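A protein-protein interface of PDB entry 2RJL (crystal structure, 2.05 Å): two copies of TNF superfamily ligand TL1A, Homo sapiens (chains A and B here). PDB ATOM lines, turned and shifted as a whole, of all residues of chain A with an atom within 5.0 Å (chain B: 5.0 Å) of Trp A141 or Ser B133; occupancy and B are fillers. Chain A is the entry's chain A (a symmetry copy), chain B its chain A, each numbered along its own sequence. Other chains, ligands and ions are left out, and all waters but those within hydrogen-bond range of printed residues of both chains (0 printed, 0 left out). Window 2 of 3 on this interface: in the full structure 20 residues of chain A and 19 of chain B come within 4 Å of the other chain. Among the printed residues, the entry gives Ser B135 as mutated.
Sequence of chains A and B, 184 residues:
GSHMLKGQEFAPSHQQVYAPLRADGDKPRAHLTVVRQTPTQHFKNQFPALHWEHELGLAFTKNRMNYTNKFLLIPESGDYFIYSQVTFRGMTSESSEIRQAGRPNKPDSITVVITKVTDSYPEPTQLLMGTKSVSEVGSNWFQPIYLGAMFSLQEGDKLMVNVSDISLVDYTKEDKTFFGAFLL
1 position is printed for both chains.
Among the printed residues, merely in contact across the chains: Trp A141 with Ser B133, Phe A142 with Thr B131, Phe A142 with Lys B132, Glu A136 with Ser B135, Gln A143 with Lys B132, Phe A142 with Ser B109, Gln A143 with Thr B131 and Glu A136 with Ser B133.
Ile A110 touches none of the printed residues of chain B.
Of the printed residues of chain B, Trp A141 touches Ser B133.
Of the printed residues of chain B, Phe A142 touches Ser B109, Thr B131, Lys B132 and Ser B133.
Printed residues of chain A within 4 Å of Lys B132: Phe A142 and Gln A143.
Printed residues of chain A within 4 Å of Ser B133: Glu A136, Trp A141 and Phe A142.
O of Phe A142 is in hydrogen-bond range of N of Ser B133 (2.9 Å).
N of Trp A141 sits close to OG of Ser A139, at 3.4 Å.
O of Trp A141 lies within hydrogen-bond range of N of Gly A90 (2.8 Å).
N of Phe A88 sits at hydrogen-bond distance from O of Gln A143 (2.7 Å).
Of the 7 printed residues of chain B, 5 touch a printed residue of chain A.
Among the printed residues, 9 pairs touch across the chains.
Among the printed residues, no Asp or Glu carboxylate lies within 4 Å of a Lys or Arg side-chain nitrogen of the other chain.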
ATOM      1  N   PHE A  88       5.232 -25.070  24.639  1.00  0.00           N
ATOM      2  CA  PHE A  88       4.340 -25.049  25.785  1.00  0.00           C
ATOM      3  C   PHE A  88       2.919 -25.083  25.233  1.00  0.00           C
ATOM      4  O   PHE A  88       2.656 -24.565  24.148  1.00  0.00           O
ATOM      5  CB  PHE A  88       4.552 -23.767  26.612  1.00  0.00           C
ATOM      6  CG  PHE A  88       5.889 -23.697  27.318  1.00  0.00           C
ATOM      7  CD1 PHE A  88       6.002 -24.061  28.652  1.00  0.00           C
ATOM      8  CD2 PHE A  88       7.022 -23.220  26.659  1.00  0.00           C
ATOM      9  CE1 PHE A  88       7.231 -23.979  29.325  1.00  0.00           C
ATOM     10  CE2 PHE A  88       8.252 -23.125  27.316  1.00  0.00           C
ATOM     11  CZ  PHE A  88       8.362 -23.513  28.652  1.00  0.00           C
ATOM     12  N   ARG A  89       2.008 -25.714  25.965  1.00  0.00           N
ATOM     13  CA  ARG A  89       0.601 -25.658  25.614  1.00  0.00           C
ATOM     14  C   ARG A  89      -0.265 -25.643  26.877  1.00  0.00           C
ATOM     15  O   ARG A  89       0.106 -26.212  27.913  1.00  0.00           O
ATOM     16  CB  ARG A  89       0.210 -26.809  24.673  1.00  0.00           C
ATOM     17  CG  ARG A  89       0.649 -28.187  25.121  1.00  0.00           C
ATOM     18  CD  ARG A  89      -0.461 -28.922  25.853  1.00  0.00           C
ATOM     19  NE  ARG A  89       0.049 -30.104  26.540  1.00  0.00           N
ATOM     20  CZ  ARG A  89       0.418 -30.132  27.816  1.00  0.00           C
ATOM     21  NH1 ARG A  89       0.871 -31.259  28.342  1.00  0.00           N
ATOM     22  NH2 ARG A  89       0.325 -29.042  28.566  1.00  0.00           N
ATOM     23  N   GLY A  90      -1.405 -24.970  26.788  1.00  0.00           N
ATOM     24  CA  GLY A  90      -2.234 -24.686  27.955  1.00  0.00           C
ATOM     25  C   GLY A  90      -3.043 -25.887  28.401  1.00  0.00           C
ATOM     26  O   GLY A  90      -3.201 -26.851  27.647  1.00  0.00           O
ATOM     27  N   PRO A 107      -1.207 -19.786  34.162  1.00  0.00           N
ATOM     28  CA  PRO A 107       0.146 -19.195  34.194  1.00  0.00           C
ATOM     29  C   PRO A 107       0.144 -17.730  33.738  1.00  0.00           C
ATOM     30  O   PRO A 107      -0.571 -17.382  32.800  1.00  0.00           O
ATOM     31  CB  PRO A 107       0.924 -20.053  33.189  1.00  0.00           C
ATOM     32  CG  PRO A 107      -0.121 -20.571  32.243  1.00  0.00           C
ATOM     33  CD  PRO A 107      -1.348 -20.793  33.090  1.00  0.00           C
ATOM     34  N   ILE A 110       5.633 -18.181  30.744  1.00  0.00           N
ATOM     35  CA  ILE A 110       6.319 -19.471  30.544  1.00  0.00           C
ATOM     36  C   ILE A 110       7.822 -19.160  30.321  1.00  0.00           C
ATOM     37  O   ILE A 110       8.160 -18.161  29.680  1.00  0.00           O
ATOM     38  CB  ILE A 110       5.741 -20.217  29.293  1.00  0.00           C
ATOM     39  CG1 ILE A 110       5.546 -19.239  28.131  1.00  0.00           C
ATOM     40  CG2 ILE A 110       4.398 -20.871  29.631  1.00  0.00           C
ATOM     41  CD1 ILE A 110       5.313 -19.902  26.745  1.00  0.00           C
ATOM     42  N   VAL A 134       2.121 -14.829  29.111  1.00  0.00           N
ATOM     43  CA  VAL A 134       1.046 -15.474  28.361  1.00  0.00           C
ATOM     44  C   VAL A 134      -0.257 -14.689  28.431  1.00  0.00           C
ATOM     45  O   VAL A 134      -0.735 -14.363  29.518  1.00  0.00           O
ATOM     46  CB  VAL A 134       0.877 -16.998  28.646  1.00  0.00           C
ATOM     47  CG1 VAL A 134       1.410 -17.374  29.997  1.00  0.00           C
ATOM     48  CG2 VAL A 134      -0.583 -17.449  28.477  1.00  0.00           C
ATOM     49  N   GLU A 136      -3.497 -14.865  26.382  1.00  0.00           N
ATOM     50  CA  GLU A 136      -4.851 -15.390  26.270  1.00  0.00           C
ATOM     51  C   GLU A 136      -5.254 -16.268  27.453  1.00  0.00           C
ATOM     52  O   GLU A 136      -4.459 -17.063  27.959  1.00  0.00           O
ATOM     53  CB  GLU A 136      -5.057 -16.116  24.934  1.00  0.00           C
ATOM     54  CG  GLU A 136      -4.296 -17.422  24.781  1.00  0.00           C
ATOM     55  CD  GLU A 136      -2.853 -17.221  24.348  1.00  0.00           C
ATOM     56  OE1 GLU A 136      -2.578 -17.285  23.129  1.00  0.00           O
ATOM     57  OE2 GLU A 136      -1.995 -17.006  25.230  1.00  0.00           O
ATOM     58  N   GLY A 138      -7.955 -19.061  29.457  1.00  0.00           N
ATOM     59  CA  GLY A 138      -8.332 -20.424  29.101  1.00  0.00           C
ATOM     60  C   GLY A 138      -7.211 -21.382  29.449  1.00  0.00           C
ATOM     61  O   GLY A 138      -7.018 -21.711  30.621  1.00  0.00           O
ATOM     62  N   SER A 139      -6.473 -21.847  28.442  1.00  0.00           N
ATOM     63  CA  SER A 139      -6.998 -22.073  27.093  1.00  0.00           C
ATOM     64  C   SER A 139      -6.378 -23.356  26.551  1.00  0.00           C
ATOM     65  O   SER A 139      -5.620 -24.028  27.255  1.00  0.00           O
ATOM     66  CB  SER A 139      -6.642 -20.908  26.166  1.00  0.00           C
ATOM     67  OG  SER A 139      -7.128 -21.133  24.854  1.00  0.00           O
ATOM     68  N   ASN A 140      -6.677 -23.694  25.301  1.00  0.00           N
ATOM     69  CA  ASN A 140      -5.741 -24.512  24.537  1.00  0.00           C
ATOM     70  C   ASN A 140      -4.867 -23.683  23.591  1.00  0.00           C
ATOM     71  O   ASN A 140      -4.800 -23.934  22.383  1.00  0.00           O
ATOM     72  CB  ASN A 140      -6.411 -25.722  23.865  1.00  0.00           C
ATOM     73  CG  ASN A 140      -7.373 -25.332  22.763  1.00  0.00           C
ATOM     74  OD1 ASN A 140      -8.561 -25.109  23.007  1.00  0.00           O
ATOM     75  ND2 ASN A 140      -6.865 -25.265  21.535  1.00  0.00           N
ATOM     76  N   TRP A 141      -4.216 -22.674  24.169  1.00  0.00           N
ATOM     77  CA  TRP A 141      -3.095 -22.005  23.532  1.00  0.00           C
ATOM     78  C   TRP A 141      -1.903 -22.942  23.425  1.00  0.00           C
ATOM     79  O   TRP A 141      -1.765 -23.896  24.201  1.00  0.00           O
ATOM     80  CB  TRP A 141      -2.718 -20.734  24.295  1.00  0.00           C
ATOM     81  CG  TRP A 141      -2.281 -20.965  25.691  1.00  0.00           C
ATOM     82  CD1 TRP A 141      -3.062 -20.922  26.814  1.00  0.00           C
ATOM     83  CD2 TRP A 141      -0.951 -21.268  26.133  1.00  0.00           C
ATOM     84  NE1 TRP A 141      -2.298 -21.185  27.929  1.00  0.00           N
ATOM     85  CE2 TRP A 141      -1.001 -21.404  27.538  1.00  0.00           C
ATOM     86  CE3 TRP A 141       0.278 -21.437  25.477  1.00  0.00           C
ATOM     87  CZ2 TRP A 141       0.130 -21.704  28.301  1.00  0.00           C
ATOM     88  CZ3 TRP A 141       1.395 -21.744  26.229  1.00  0.00           C
ATOM     89  CH2 TRP A 141       1.316 -21.861  27.635  1.00  0.00           C
ATOM     90  N   PHE A 142      -1.039 -22.673  22.456  1.00  0.00           N
ATOM     91  CA  PHE A 142       0.262 -23.331  22.415  1.00  0.00           C
ATOM     92  C   PHE A 142       1.282 -22.429  21.765  1.00  0.00           C
ATOM     93  O   PHE A 142       0.946 -21.602  20.912  1.00  0.00           O
ATOM     94  CB  PHE A 142       0.224 -24.713  21.748  1.00  0.00           C
ATOM     95  CG  PHE A 142      -0.587 -24.771  20.486  1.00  0.00           C
ATOM     96  CD1 PHE A 142      -1.935 -25.109  20.528  1.00  0.00           C
ATOM     97  CD2 PHE A 142       0.000 -24.517  19.258  1.00  0.00           C
ATOM     98  CE1 PHE A 142      -2.699 -25.174  19.360  1.00  0.00           C
ATOM     99  CE2 PHE A 142      -0.752 -24.584  18.077  1.00  0.00           C
ATOM    100  CZ  PHE A 142      -2.103 -24.913  18.131  1.00  0.00           C
ATOM    101  N   GLN A 143       2.525 -22.566  22.208  1.00  0.00           N
ATOM    102  CA  GLN A 143       3.612 -21.821  21.613  1.00  0.00           C
ATOM    103  C   GLN A 143       5.011 -22.298  22.016  1.00  0.00           C
ATOM    104  O   GLN A 143       5.217 -22.798  23.138  1.00  0.00           O
ATOM    105  CB  GLN A 143       3.446 -20.354  21.933  1.00  0.00           C
ATOM    106  CG  GLN A 143       3.624 -20.027  23.373  1.00  0.00           C
ATOM    107  CD  GLN A 143       3.260 -18.581  23.621  1.00  0.00           C
ATOM    108  OE1 GLN A 143       3.748 -17.696  22.927  1.00  0.00           O
ATOM    109  NE2 GLN A 143       2.384 -18.335  24.589  1.00  0.00           N
ATOM    110  N   LEU A 168       3.055 -27.848  31.554  1.00  0.00           N
ATOM    111  CA  LEU A 168       2.716 -27.125  30.317  1.00  0.00           C
ATOM    112  C   LEU A 168       3.564 -27.538  29.114  1.00  0.00           C
ATOM    113  O   LEU A 168       3.318 -27.098  28.000  1.00  0.00           O
ATOM    114  CB  LEU A 168       2.848 -25.621  30.523  1.00  0.00           C
ATOM    115  CG  LEU A 168       1.947 -24.977  31.580  1.00  0.00           C
ATOM    116  CD1 LEU A 168       2.297 -23.512  31.674  1.00  0.00           C
ATOM    117  CD2 LEU A 168       0.474 -25.159  31.198  1.00  0.00           C
ATOM    118  N   ASP B 108      -6.759 -20.526  13.338  1.00  0.00           N
ATOM    119  CA  ASP B 108      -6.600 -20.782  14.770  1.00  0.00           C
ATOM    120  C   ASP B 108      -5.131 -20.923  15.207  1.00  0.00           C
ATOM    121  O   ASP B 108      -4.805 -20.764  16.392  1.00  0.00           O
ATOM    122  CB  ASP B 108      -7.372 -22.036  15.177  1.00  0.00           C
ATOM    123  CG  ASP B 108      -8.879 -21.845  15.104  1.00  0.00           C
ATOM    124  OD1 ASP B 108      -9.373 -20.787  15.551  1.00  0.00           O
ATOM    125  OD2 ASP B 108      -9.569 -22.756  14.599  1.00  0.00           O
ATOM    126  N   SER B 109      -4.259 -21.239  14.254  1.00  0.00           N
ATOM    127  CA  SER B 109      -2.847 -21.467  14.540  1.00  0.00           C
ATOM    128  C   SER B 109      -2.037 -21.347  13.258  1.00  0.00           C
ATOM    129  O   SER B 109      -2.596 -21.358  12.142  1.00  0.00           O
ATOM    130  CB  SER B 109      -2.654 -22.854  15.158  1.00  0.00           C
ATOM    131  OG  SER B 109      -2.933 -23.844  14.186  1.00  0.00           O
ATOM    132  N   THR B 131       4.872 -24.471  16.111  1.00  0.00           N
ATOM    133  CA  THR B 131       3.438 -24.272  15.939  1.00  0.00           C
ATOM    134  C   THR B 131       2.952 -23.345  17.035  1.00  0.00           C
ATOM    135  O   THR B 131       3.329 -23.479  18.208  1.00  0.00           O
ATOM    136  CB  THR B 131       2.660 -25.642  15.860  1.00  0.00           C
ATOM    137  OG1 THR B 131       1.281 -25.409  15.547  1.00  0.00           O
ATOM    138  CG2 THR B 131       2.767 -26.430  17.164  1.00  0.00           C
ATOM    139  N   LYS B 132       2.158 -22.363  16.645  1.00  0.00           N
ATOM    140  CA  LYS B 132       1.743 -21.332  17.578  1.00  0.00           C
ATOM    141  C   LYS B 132       0.243 -21.066  17.401  1.00  0.00           C
ATOM    142  O   LYS B 132      -0.216 -20.934  16.287  1.00  0.00           O
ATOM    143  CB  LYS B 132       2.516 -20.053  17.302  1.00  0.00           C
ATOM    144  CG  LYS B 132       2.233 -18.968  18.311  1.00  0.00           C
ATOM    145  CD  LYS B 132       3.393 -17.995  18.423  1.00  0.00           C
ATOM    146  CE  LYS B 132       3.109 -16.979  19.512  1.00  0.00           C
ATOM    147  NZ  LYS B 132       1.711 -16.472  19.401  1.00  0.00           N
ATOM    148  N   SER B 133      -0.524 -21.002  18.489  1.00  0.00           N
ATOM    149  CA  SER B 133      -1.937 -20.615  18.372  1.00  0.00           C
ATOM    150  C   SER B 133      -2.021 -19.115  18.122  1.00  0.00           C
ATOM    151  O   SER B 133      -1.221 -18.358  18.666  1.00  0.00           O
ATOM    152  CB  SER B 133      -2.717 -21.007  19.635  1.00  0.00           C
ATOM    153  OG  SER B 133      -2.097 -20.484  20.790  1.00  0.00           O
ATOM    154  N   VAL B 134      -2.947 -18.670  17.270  1.00  0.00           N
ATOM    155  CA  VAL B 134      -3.022 -17.233  17.013  1.00  0.00           C
ATOM    156  C   VAL B 134      -4.181 -16.576  17.752  1.00  0.00           C
ATOM    157  O   VAL B 134      -5.326 -17.013  17.637  1.00  0.00           O
ATOM    158  CB  VAL B 134      -2.931 -16.835  15.508  1.00  0.00           C
ATOM    159  CG1 VAL B 134      -3.367 -17.955  14.609  1.00  0.00           C
ATOM    160  CG2 VAL B 134      -3.714 -15.546  15.212  1.00  0.00           C
ATOM    161  N   SER B 135      -3.849 -15.542  18.525  1.00  0.00           N
ATOM    162  CA  SER B 135      -4.709 -15.047  19.600  1.00  0.00           C
ATOM    163  C   SER B 135      -5.620 -13.942  19.097  1.00  0.00           C
ATOM    164  O   SER B 135      -6.841 -14.026  19.228  1.00  0.00           O
ATOM    165  CB  SER B 135      -3.866 -14.518  20.766  1.00  0.00           C
ATOM    166  OG  SER B 135      -2.499 -14.851  20.609  1.00  0.00           O
